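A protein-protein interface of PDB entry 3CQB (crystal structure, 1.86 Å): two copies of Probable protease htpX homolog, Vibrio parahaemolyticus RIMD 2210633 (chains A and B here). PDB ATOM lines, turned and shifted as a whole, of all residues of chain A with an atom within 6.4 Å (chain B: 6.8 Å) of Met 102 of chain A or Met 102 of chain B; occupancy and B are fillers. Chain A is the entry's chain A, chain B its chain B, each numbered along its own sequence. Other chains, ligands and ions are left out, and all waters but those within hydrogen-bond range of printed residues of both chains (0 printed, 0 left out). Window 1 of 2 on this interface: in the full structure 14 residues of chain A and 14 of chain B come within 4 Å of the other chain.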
ATOM      1  N   ILE A  54       5.677 -11.187 -18.201  1.00  0.00           N
ATOM      2  CA  ILE A  54       6.345 -12.054 -19.163  1.00  0.00           C
ATOM      3  C   ILE A  54       7.759 -12.267 -18.614  1.00  0.00           C
ATOM      4  O   ILE A  54       8.591 -11.361 -18.673  1.00  0.00           O
ATOM      5  CB  ILE A  54       6.398 -11.387 -20.564  1.00  0.00           C
ATOM      6  CG1 ILE A  54       4.960 -11.163 -21.083  1.00  0.00           C
ATOM      7  CG2 ILE A  54       7.260 -12.250 -21.533  1.00  0.00           C
ATOM      8  CD1 ILE A  54       4.831 -10.028 -22.151  1.00  0.00           C
ATOM      9  N   ASN A  55       8.033 -13.450 -18.082  1.00  0.00           N
ATOM     10  CA  ASN A  55       9.327 -13.675 -17.445  1.00  0.00           C
ATOM     11  C   ASN A  55       9.702 -15.143 -17.544  1.00  0.00           C
ATOM     12  O   ASN A  55       8.831 -16.017 -17.484  1.00  0.00           O
ATOM     13  CB  ASN A  55       9.262 -13.271 -15.963  1.00  0.00           C
ATOM     14  CG  ASN A  55      10.485 -13.756 -15.176  1.00  0.00           C
ATOM     15  OD1 ASN A  55      10.538 -14.906 -14.699  1.00  0.00           O
ATOM     16  ND2 ASN A  55      11.479 -12.873 -15.042  1.00  0.00           N
ATOM     17  N   ALA A  56      10.992 -15.421 -17.693  1.00  0.00           N
ATOM     18  CA  ALA A  56      11.516 -16.760 -17.442  1.00  0.00           C
ATOM     19  C   ALA A  56      12.727 -16.582 -16.541  1.00  0.00           C
ATOM     20  O   ALA A  56      13.498 -15.602 -16.682  1.00  0.00           O
ATOM     21  CB  ALA A  56      11.945 -17.433 -18.778  1.00  0.00           C
ATOM     22  N   PHE A  57      12.907 -17.504 -15.603  1.00  0.00           N
ATOM     23  CA  PHE A  57      14.134 -17.498 -14.808  1.00  0.00           C
ATOM     24  C   PHE A  57      14.715 -18.874 -14.684  1.00  0.00           C
ATOM     25  O   PHE A  57      13.991 -19.878 -14.852  1.00  0.00           O
ATOM     26  CB  PHE A  57      13.947 -16.842 -13.438  1.00  0.00           C
ATOM     27  CG  PHE A  57      12.980 -17.562 -12.489  1.00  0.00           C
ATOM     28  CD1 PHE A  57      13.470 -18.498 -11.568  1.00  0.00           C
ATOM     29  CD2 PHE A  57      11.604 -17.203 -12.441  1.00  0.00           C
ATOM     30  CE1 PHE A  57      12.600 -19.119 -10.632  1.00  0.00           C
ATOM     31  CE2 PHE A  57      10.734 -17.806 -11.496  1.00  0.00           C
ATOM     32  CZ  PHE A  57      11.228 -18.761 -10.601  1.00  0.00           C
ATOM     33  N   LEU A  74       4.398 -15.152 -20.233  1.00  0.00           N
ATOM     34  CA  LEU A  74       5.355 -15.395 -21.325  1.00  0.00           C
ATOM     35  C   LEU A  74       4.741 -16.339 -22.392  1.00  0.00           C
ATOM     36  O   LEU A  74       4.751 -16.044 -23.607  1.00  0.00           O
ATOM     37  CB  LEU A  74       6.673 -15.966 -20.755  1.00  0.00           C
ATOM     38  CG  LEU A  74       7.783 -16.156 -21.805  1.00  0.00           C
ATOM     39  CD1 LEU A  74       9.160 -15.956 -21.146  1.00  0.00           C
ATOM     40  CD2 LEU A  74       7.678 -17.499 -22.534  1.00  0.00           C
ATOM     41  N   ALA A  85      13.953 -18.840 -28.201  1.00  0.00           N
ATOM     42  CA  ALA A  85      15.187 -18.031 -28.170  1.00  0.00           C
ATOM     43  C   ALA A  85      15.518 -17.580 -26.727  1.00  0.00           C
ATOM     44  O   ALA A  85      16.683 -17.580 -26.299  1.00  0.00           O
ATOM     45  CB  ALA A  85      15.075 -16.840 -29.093  1.00  0.00           C
ATOM     46  N   VAL A  86      14.492 -17.242 -25.959  1.00  0.00           N
ATOM     47  CA  VAL A  86      14.676 -16.833 -24.565  1.00  0.00           C
ATOM     48  C   VAL A  86      15.199 -18.025 -23.763  1.00  0.00           C
ATOM     49  O   VAL A  86      16.169 -17.913 -22.976  1.00  0.00           O
ATOM     50  CB  VAL A  86      13.353 -16.290 -23.955  1.00  0.00           C
ATOM     51  CG1 VAL A  86      13.456 -16.175 -22.394  1.00  0.00           C
ATOM     52  CG2 VAL A  86      13.038 -14.921 -24.540  1.00  0.00           C
ATOM     53  N   LEU A  87      14.572 -19.181 -23.969  1.00  0.00           N
ATOM     54  CA  LEU A  87      14.974 -20.379 -23.245  1.00  0.00           C
ATOM     55  C   LEU A  87      16.413 -20.783 -23.594  1.00  0.00           C
ATOM     56  O   LEU A  87      17.199 -21.136 -22.708  1.00  0.00           O
ATOM     57  CB  LEU A  87      13.981 -21.523 -23.531  1.00  0.00           C
ATOM     58  CG  LEU A  87      12.556 -21.336 -22.983  1.00  0.00           C
ATOM     59  CD1 LEU A  87      11.607 -22.372 -23.638  1.00  0.00           C
ATOM     60  CD2 LEU A  87      12.625 -21.498 -21.478  1.00  0.00           C
ATOM     61  N   HIS A  89      18.818 -18.892 -24.516  1.00  0.00           N
ATOM     62  CA  HIS A  89      19.718 -17.938 -23.872  1.00  0.00           C
ATOM     63  C   HIS A  89      19.875 -18.239 -22.376  1.00  0.00           C
ATOM     64  O   HIS A  89      21.009 -18.270 -21.861  1.00  0.00           O
ATOM     65  CB  HIS A  89      19.294 -16.475 -24.117  1.00  0.00           C
ATOM     66  CG  HIS A  89      20.336 -15.498 -23.675  1.00  0.00           C
ATOM     67  ND1 HIS A  89      21.548 -15.358 -24.327  1.00  0.00           N
ATOM     68  CD2 HIS A  89      20.400 -14.694 -22.586  1.00  0.00           C
ATOM     69  CE1 HIS A  89      22.294 -14.475 -23.682  1.00  0.00           C
ATOM     70  NE2 HIS A  89      21.616 -14.044 -22.632  1.00  0.00           N
ATOM     71  N   GLU A  90      18.764 -18.506 -21.697  1.00  0.00           N
ATOM     72  CA  GLU A  90      18.827 -18.905 -20.277  1.00  0.00           C
ATOM     73  C   GLU A  90      19.546 -20.213 -20.034  1.00  0.00           C
ATOM     74  O   GLU A  90      20.330 -20.312 -19.073  1.00  0.00           O
ATOM     75  CB  GLU A  90      17.441 -18.876 -19.611  1.00  0.00           C
ATOM     76  CG  GLU A  90      16.841 -17.473 -19.692  1.00  0.00           C
ATOM     77  CD  GLU A  90      15.792 -17.171 -18.632  1.00  0.00           C
ATOM     78  OE1 GLU A  90      15.382 -18.108 -17.905  1.00  0.00           O
ATOM     79  OE2 GLU A  90      15.400 -15.971 -18.507  1.00  0.00           O
ATOM     80  N   HIS A  93      23.239 -19.657 -19.775  1.00  0.00           N
ATOM     81  CA  HIS A  93      23.635 -19.216 -18.441  1.00  0.00           C
ATOM     82  C   HIS A  93      23.710 -20.340 -17.436  1.00  0.00           C
ATOM     83  O   HIS A  93      24.668 -20.406 -16.643  1.00  0.00           O
ATOM     84  CB  HIS A  93      22.705 -18.078 -17.954  1.00  0.00           C
ATOM     85  CG  HIS A  93      22.884 -16.826 -18.744  1.00  0.00           C
ATOM     86  ND1 HIS A  93      24.100 -16.180 -18.816  1.00  0.00           N
ATOM     87  CD2 HIS A  93      22.036 -16.139 -19.548  1.00  0.00           C
ATOM     88  CE1 HIS A  93      23.993 -15.146 -19.632  1.00  0.00           C
ATOM     89  NE2 HIS A  93      22.746 -15.093 -20.082  1.00  0.00           N
ATOM     90  N   VAL A 100      19.802 -16.586 -13.886  1.00  0.00           N
ATOM     91  CA  VAL A 100      19.369 -15.507 -14.764  1.00  0.00           C
ATOM     92  C   VAL A 100      17.866 -15.308 -14.605  1.00  0.00           C
ATOM     93  O   VAL A 100      17.137 -16.299 -14.395  1.00  0.00           O
ATOM     94  CB  VAL A 100      19.687 -15.818 -16.259  1.00  0.00           C
ATOM     95  CG1 VAL A 100      19.170 -17.259 -16.696  1.00  0.00           C
ATOM     96  CG2 VAL A 100      19.078 -14.722 -17.179  1.00  0.00           C
ATOM     97  N   THR A 101      17.414 -14.063 -14.718  1.00  0.00           N
ATOM     98  CA  THR A 101      15.988 -13.805 -14.819  1.00  0.00           C
ATOM     99  C   THR A 101      15.783 -12.749 -15.898  1.00  0.00           C
ATOM    100  O   THR A 101      16.618 -11.857 -16.051  1.00  0.00           O
ATOM    101  CB  THR A 101      15.383 -13.399 -13.445  1.00  0.00           C
ATOM    102  OG1 THR A 101      13.983 -13.201 -13.593  1.00  0.00           O
ATOM    103  CG2 THR A 101      16.027 -12.089 -12.888  1.00  0.00           C
ATOM    104  N   MET A 102      14.725 -12.880 -16.698  1.00  0.00           N
ATOM    105  CA  MET A 102      14.552 -11.960 -17.824  1.00  0.00           C
ATOM    106  C   MET A 102      13.089 -11.663 -17.950  1.00  0.00           C
ATOM    107  O   MET A 102      12.255 -12.602 -18.015  1.00  0.00           O
ATOM    108  CB  MET A 102      15.031 -12.607 -19.132  1.00  0.00           C
ATOM    109  CG  MET A 102      15.167 -11.626 -20.297  1.00  0.00           C
ATOM    110  SD  MET A 102      15.457 -12.523 -22.028  1.00  0.00           S
ATOM    111  CE  MET A 102      16.716 -13.890 -21.500  1.00  0.00           C
ATOM    112  N   THR A 103      12.768 -10.375 -18.018  1.00  0.00           N
ATOM    113  CA  THR A 103      11.369  -9.957 -18.092  1.00  0.00           C
ATOM    114  C   THR A 103      11.217  -9.111 -19.339  1.00  0.00           C
ATOM    115  O   THR A 103      12.118  -8.303 -19.654  1.00  0.00           O
ATOM    116  CB  THR A 103      10.953  -9.156 -16.814  1.00  0.00           C
ATOM    117  OG1 THR A 103      11.150  -9.984 -15.655  1.00  0.00           O
ATOM    118  CG2 THR A 103       9.467  -8.693 -16.882  1.00  0.00           C
ATOM    119  N   LEU A 104      10.104  -9.290 -20.059  1.00  0.00           N
ATOM    120  CA  LEU A 104       9.800  -8.455 -21.230  1.00  0.00           C
ATOM    121  C   LEU A 104       8.578  -7.600 -20.946  1.00  0.00           C
ATOM    122  O   LEU A 104       7.685  -8.015 -20.207  1.00  0.00           O
ATOM    123  CB  LEU A 104       9.440  -9.296 -22.454  1.00  0.00           C
ATOM    124  CG  LEU A 104      10.461  -9.968 -23.363  1.00  0.00           C
ATOM    125  CD1 LEU A 104      10.814  -9.074 -24.551  1.00  0.00           C
ATOM    126  CD2 LEU A 104      11.686 -10.444 -22.631  1.00  0.00           C
ATOM    127  N   ILE B  54      24.096  -7.099 -11.817  1.00  0.00           N
ATOM    128  CA  ILE B  54      24.545  -7.358 -13.180  1.00  0.00           C
ATOM    129  C   ILE B  54      23.276  -7.324 -14.048  1.00  0.00           C
ATOM    130  O   ILE B  54      22.502  -8.278 -14.060  1.00  0.00           O
ATOM    131  CB  ILE B  54      25.227  -8.737 -13.291  1.00  0.00           C
ATOM    132  CG1 ILE B  54      26.481  -8.805 -12.397  1.00  0.00           C
ATOM    133  CG2 ILE B  54      25.522  -9.063 -14.794  1.00  0.00           C
ATOM    134  CD1 ILE B  54      26.979 -10.306 -12.207  1.00  0.00           C
ATOM    135  N   ASN B  55      23.050  -6.211 -14.744  1.00  0.00           N
ATOM    136  CA  ASN B  55      21.784  -6.002 -15.462  1.00  0.00           C
ATOM    137  C   ASN B  55      22.022  -5.259 -16.752  1.00  0.00           C
ATOM    138  O   ASN B  55      22.864  -4.363 -16.816  1.00  0.00           O
ATOM    139  CB  ASN B  55      20.774  -5.207 -14.589  1.00  0.00           C
ATOM    140  CG  ASN B  55      19.507  -4.819 -15.371  1.00  0.00           C
ATOM    141  OD1 ASN B  55      18.593  -5.658 -15.539  1.00  0.00           O
ATOM    142  ND2 ASN B  55      19.453  -3.603 -15.879  1.00  0.00           N
ATOM    143  N   ALA B  56      21.271  -5.629 -17.797  1.00  0.00           N
ATOM    144  CA  ALA B  56      21.181  -4.784 -18.969  1.00  0.00           C
ATOM    145  C   ALA B  56      19.693  -4.709 -19.305  1.00  0.00           C
ATOM    146  O   ALA B  56      18.956  -5.722 -19.180  1.00  0.00           O
ATOM    147  CB  ALA B  56      21.956  -5.399 -20.159  1.00  0.00           C
ATOM    148  N   PHE B  57      19.261  -3.529 -19.731  1.00  0.00           N
ATOM    149  CA  PHE B  57      17.906  -3.409 -20.279  1.00  0.00           C
ATOM    150  C   PHE B  57      17.915  -2.647 -21.594  1.00  0.00           C
ATOM    151  O   PHE B  57      18.853  -1.907 -21.886  1.00  0.00           O
ATOM    152  CB  PHE B  57      16.889  -2.869 -19.270  1.00  0.00           C
ATOM    153  CG  PHE B  57      17.031  -1.400 -18.948  1.00  0.00           C
ATOM    154  CD1 PHE B  57      17.720  -0.998 -17.797  1.00  0.00           C
ATOM    155  CD2 PHE B  57      16.427  -0.442 -19.743  1.00  0.00           C
ATOM    156  CE1 PHE B  57      17.813   0.359 -17.450  1.00  0.00           C
ATOM    157  CE2 PHE B  57      16.510   0.920 -19.417  1.00  0.00           C
ATOM    158  CZ  PHE B  57      17.217   1.318 -18.272  1.00  0.00           C
ATOM    159  N   ALA B  58      16.909  -2.893 -22.418  1.00  0.00           N
ATOM    160  CA  ALA B  58      16.931  -2.368 -23.771  1.00  0.00           C
ATOM    161  C   ALA B  58      15.492  -2.221 -24.216  1.00  0.00           C
ATOM    162  O   ALA B  58      14.613  -2.961 -23.763  1.00  0.00           O
ATOM    163  CB  ALA B  58      17.657  -3.325 -24.704  1.00  0.00           C
ATOM    164  N   LEU B  74      27.257  -4.800 -14.228  1.00  0.00           N
ATOM    165  CA  LEU B  74      27.523  -5.659 -15.397  1.00  0.00           C
ATOM    166  C   LEU B  74      28.946  -5.442 -15.943  1.00  0.00           C
ATOM    167  O   LEU B  74      29.721  -6.409 -16.124  1.00  0.00           O
ATOM    168  CB  LEU B  74      26.454  -5.444 -16.473  1.00  0.00           C
ATOM    169  CG  LEU B  74      26.636  -6.365 -17.705  1.00  0.00           C
ATOM    170  CD1 LEU B  74      25.267  -6.652 -18.333  1.00  0.00           C
ATOM    171  CD2 LEU B  74      27.587  -5.732 -18.708  1.00  0.00           C
ATOM    172  N   ALA B  85      27.312 -11.557 -25.362  1.00  0.00           N
ATOM    173  CA  ALA B  85      26.210 -12.527 -25.520  1.00  0.00           C
ATOM    174  C   ALA B  85      24.889 -11.957 -24.985  1.00  0.00           C
ATOM    175  O   ALA B  85      23.815 -12.057 -25.642  1.00  0.00           O
ATOM    176  CB  ALA B  85      26.550 -13.869 -24.859  1.00  0.00           C
ATOM    177  N   VAL B  86      24.937 -11.354 -23.803  1.00  0.00           N
ATOM    178  CA  VAL B  86      23.758 -10.719 -23.234  1.00  0.00           C
ATOM    179  C   VAL B  86      23.258  -9.609 -24.147  1.00  0.00           C
ATOM    180  O   VAL B  86      22.046  -9.522 -24.426  1.00  0.00           O
ATOM    181  CB  VAL B  86      24.049 -10.155 -21.809  1.00  0.00           C
ATOM    182  CG1 VAL B  86      22.909  -9.253 -21.302  1.00  0.00           C
ATOM    183  CG2 VAL B  86      24.320 -11.301 -20.849  1.00  0.00           C
ATOM    184  N   LEU B  87      24.172  -8.750 -24.617  1.00  0.00           N
ATOM    185  CA  LEU B  87      23.751  -7.610 -25.428  1.00  0.00           C
ATOM    186  C   LEU B  87      23.156  -8.088 -26.761  1.00  0.00           C
ATOM    187  O   LEU B  87      22.163  -7.530 -27.247  1.00  0.00           O
ATOM    188  CB  LEU B  87      24.929  -6.663 -25.673  1.00  0.00           C
ATOM    189  CG  LEU B  87      25.419  -5.921 -24.403  1.00  0.00           C
ATOM    190  CD1 LEU B  87      26.778  -5.225 -24.709  1.00  0.00           C
ATOM    191  CD2 LEU B  87      24.357  -4.943 -23.922  1.00  0.00           C
ATOM    192  N   HIS B  89      21.557 -10.800 -27.358  1.00  0.00           N
ATOM    193  CA  HIS B  89      20.195 -11.268 -27.108  1.00  0.00           C
ATOM    194  C   HIS B  89      19.244 -10.076 -26.918  1.00  0.00           C
ATOM    195  O   HIS B  89      18.126 -10.063 -27.464  1.00  0.00           O
ATOM    196  CB  HIS B  89      20.132 -12.202 -25.883  1.00  0.00           C
ATOM    197  CG  HIS B  89      18.789 -12.842 -25.727  1.00  0.00           C
ATOM    198  ND1 HIS B  89      18.325 -13.796 -26.608  1.00  0.00           N
ATOM    199  CD2 HIS B  89      17.777 -12.605 -24.859  1.00  0.00           C
ATOM    200  CE1 HIS B  89      17.096 -14.151 -26.266  1.00  0.00           C
ATOM    201  NE2 HIS B  89      16.742 -13.453 -25.200  1.00  0.00           N
ATOM    202  N   GLU B  90      19.679  -9.055 -26.180  1.00  0.00           N
ATOM    203  CA  GLU B  90      18.792  -7.904 -25.954  1.00  0.00           C
ATOM    204  C   GLU B  90      18.524  -7.103 -27.221  1.00  0.00           C
ATOM    205  O   GLU B  90      17.392  -6.643 -27.450  1.00  0.00           O
ATOM    206  CB  GLU B  90      19.329  -7.019 -24.844  1.00  0.00           C
ATOM    207  CG  GLU B  90      19.253  -7.738 -23.506  1.00  0.00           C
ATOM    208  CD  GLU B  90      19.198  -6.826 -22.286  1.00  0.00           C
ATOM    209  OE1 GLU B  90      19.365  -5.581 -22.426  1.00  0.00           O
ATOM    210  OE2 GLU B  90      18.968  -7.386 -21.162  1.00  0.00           O
ATOM    211  N   HIS B  93      15.640  -8.457 -29.111  1.00  0.00           N
ATOM    212  CA  HIS B  93      14.372  -7.944 -28.587  1.00  0.00           C
ATOM    213  C   HIS B  93      14.052  -6.532 -29.059  1.00  0.00           C
ATOM    214  O   HIS B  93      12.927  -6.265 -29.462  1.00  0.00           O
ATOM    215  CB  HIS B  93      14.355  -8.042 -27.050  1.00  0.00           C
ATOM    216  CG  HIS B  93      14.305  -9.462 -26.564  1.00  0.00           C
ATOM    217  ND1 HIS B  93      13.217 -10.278 -26.790  1.00  0.00           N
ATOM    218  CD2 HIS B  93      15.218 -10.223 -25.917  1.00  0.00           C
ATOM    219  CE1 HIS B  93      13.452 -11.475 -26.278  1.00  0.00           C
ATOM    220  NE2 HIS B  93      14.656 -11.469 -25.734  1.00  0.00           N
ATOM    221  N   VAL B 100      13.185  -5.278 -22.844  1.00  0.00           N
ATOM    222  CA  VAL B 100      13.671  -6.472 -22.152  1.00  0.00           C
ATOM    223  C   VAL B 100      14.573  -6.020 -21.027  1.00  0.00           C
ATOM    224  O   VAL B 100      15.292  -5.008 -21.152  1.00  0.00           O
ATOM    225  CB  VAL B 100      14.430  -7.418 -23.108  1.00  0.00           C
ATOM    226  CG1 VAL B 100      15.615  -6.676 -23.830  1.00  0.00           C
ATOM    227  CG2 VAL B 100      14.933  -8.667 -22.380  1.00  0.00           C
ATOM    228  N   THR B 101      14.540  -6.754 -19.924  1.00  0.00           N
ATOM    229  CA  THR B 101      15.536  -6.515 -18.868  1.00  0.00           C
ATOM    230  C   THR B 101      16.020  -7.877 -18.409  1.00  0.00           C
ATOM    231  O   THR B 101      15.217  -8.828 -18.309  1.00  0.00           O
ATOM    232  CB  THR B 101      14.934  -5.670 -17.704  1.00  0.00           C
ATOM    233  OG1 THR B 101      15.896  -5.544 -16.653  1.00  0.00           O
ATOM    234  CG2 THR B 101      13.644  -6.340 -17.110  1.00  0.00           C
ATOM    235  N   MET B 102      17.318  -7.996 -18.147  1.00  0.00           N
ATOM    236  CA  MET B 102      17.873  -9.290 -17.773  1.00  0.00           C
ATOM    237  C   MET B 102      18.818  -9.057 -16.626  1.00  0.00           C
ATOM    238  O   MET B 102      19.676  -8.161 -16.709  1.00  0.00           O
ATOM    239  CB  MET B 102      18.660  -9.894 -18.937  1.00  0.00           C
ATOM    240  CG  MET B 102      18.961 -11.384 -18.750  1.00  0.00           C
ATOM    241  SD  MET B 102      20.198 -12.094 -20.076  1.00  0.00           S
ATOM    242  CE  MET B 102      19.461 -11.230 -21.676  1.00  0.00           C
ATOM    243  N   THR B 103      18.718  -9.890 -15.594  1.00  0.00           N
ATOM    244  CA  THR B 103      19.614  -9.747 -14.462  1.00  0.00           C
ATOM    245  C   THR B 103      20.262 -11.095 -14.205  1.00  0.00           C
ATOM    246  O   THR B 103      19.585 -12.144 -14.292  1.00  0.00           O
ATOM    247  CB  THR B 103      18.859  -9.232 -13.217  1.00  0.00           C
ATOM    248  OG1 THR B 103      18.249  -7.967 -13.547  1.00  0.00           O
ATOM    249  CG2 THR B 103      19.815  -9.027 -12.024  1.00  0.00           C
ATOM    250  N   LEU B 104      21.565 -11.065 -13.914  1.00  0.00           N
ATOM    251  CA  LEU B 104      22.334 -12.291 -13.713  1.00  0.00           C
ATOM    252  C   LEU B 104      23.007 -12.331 -12.354  1.00  0.00           C
ATOM    253  O   LEU B 104      23.306 -11.281 -11.770  1.00  0.00           O
ATOM    254  CB  LEU B 104      23.442 -12.433 -14.777  1.00  0.00           C
ATOM    255  CG  LEU B 104      23.103 -12.278 -16.269  1.00  0.00           C
ATOM    256  CD1 LEU B 104      24.381 -12.415 -17.049  1.00  0.00           C
ATOM    257  CD2 LEU B 104      22.219 -13.391 -16.686  1.00  0.00           C
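The side-chain sulfur (SD) of Met 102 of chain B lies within hydrogen-bond range of a ring nitrogen (NE2) of His 89 of chain A (3.5 Å).
O of Thr 101 of chain A is in hydrogen-bond range of N of Thr 103 of chain B (2.9 Å).
SD of Met 102 of chain A sits at hydrogen-bond distance from NE2 of His 89 of chain B, at 3.5 Å.
The backbone NH (N) of Thr 101 of chain B sits at hydrogen-bond distance from the backbone carbonyl oxygen (O) of Thr 103 of chain A, at 2.9 Å.
ND2 of Asn 55 of chain A lies within hydrogen-bond range of OG1 of Thr 103 of chain A.
The side-chain amide oxygen (OD1) of Asn 55 of chain B sits at hydrogen-bond distance from the side-chain hydroxyl (OG1) of Thr 101 of chain B (2.9 Å).
The backbone carbonyl oxygen (O) of Met 102 of chain B sits close to the side-chain amide oxygen (OD1) of Asn 55 of chain B, at 3.0 Å.
OD1 of Asn 55 of chain B is in hydrogen-bond range of OG1 of Thr 103 of chain B (3.1 Å).
The backbone NH of Met 102 of chain B is in hydrogen-bond range of the backbone carbonyl oxygen of Ala 56 of chain B, 3.0 Å away.
N of Val 100 of chain B lies within hydrogen-bond range of O of Ala 58 of chain B (2.9 Å).
Among the printed residues, merely in contact across the chains: Met 102 of chain A with Thr 101 of chain B, Thr 101 of chain A with Met 102 of chain B, Val 100 of chain A with Thr 103 of chain B, Val 100 of chain A with Leu 104 of chain B, Ala 85 of chain A with His 89 of chain B, His 89 of chain A with Ala 85 of chain B, Thr 103 of chain A with Val 100 of chain B, Leu 104 of chain A with His 93 of chain B, Met 102 of chain A with Val 100 of chain B, Val 100 of chain A with Met 102 of chain B, His 89 of chain A with His 89 of chain B, Leu 104 of chain A with Val 100 of chain B, His 93 of chain A with Leu 104 of chain B, Met 102 of chain A with Met 102 of chain B, Val 86 of chain A with His 93 of chain B, His 93 of chain A with Met 102 of chain B, Met 102 of chain A with His 93 of chain B and Val 86 of chain A with His 89 of chain B.
Of chain B, only His 89, His 93, Val 100, Thr 101 and Met 102 come within 4 Å of Met 102 of chain A.
Printed residues of chain A within 4 Å of His 89 of chain B: Ala 85, Val 86, His 89 and Met 102.
Printed residues of chain A within 4 Å of Thr 101 of chain B: Met 102 (3.2 Å) and Thr 103 (2.9 Å).
Met 102 of chain B touches just these residues of chain A: His 89, His 93, Val 100, Thr 101 and Met 102.
Of the printed residues of chain A, Leu 104 of chain B touches His 93 (3.8 Å) and Val 100 (3.4 Å).
The nearest residue of chain B that does not touch Met 102 of chain A is Thr 103 of chain B (5.1 Å).
The nearest printed residue of chain B that does not touch Leu 104 of chain A is Thr 101 of chain B (5.1 Å).
Of the 16 printed residues of chain A, 9 touch a printed residue of chain B.
Of the 17 printed residues of chain B, 8 touch a printed residue of chain A.
Printed residues of chain B that touch a printed residue of chain A: Ala 85, His 89, His 93, Val 100, Thr 101, Met 102, Thr 103 and Leu 104.
Among the printed residues, 22 pairs touch across the chains.
Among the printed residues, no Asp or Glu carboxylate lies within 4 Å of a Lys or Arg side-chain nitrogen of the other chain.
Ala 85 of chain A touches His 89 of chain B, and with the chains exchanged His 89 of chain A touches Ala 85 of chain B.
Val 86 of chain A touches His 93 of chain B, but with the chains exchanged His 93 of chain A does not touch Val 86 of chain B (4.05 Å).
His 93 of chain A touches Met 102 of chain B, and with the chains exchanged Met 102 of chain A touches His 93 of chain B.
Thr 101 of chain A touches Met 102 of chain B, and with the chains exchanged Met 102 of chain A touches Thr 101 of chain B.
Of the 22 pairs that touch across the chains among the printed residues, 20 have their exchanged pair printed and touching as well.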
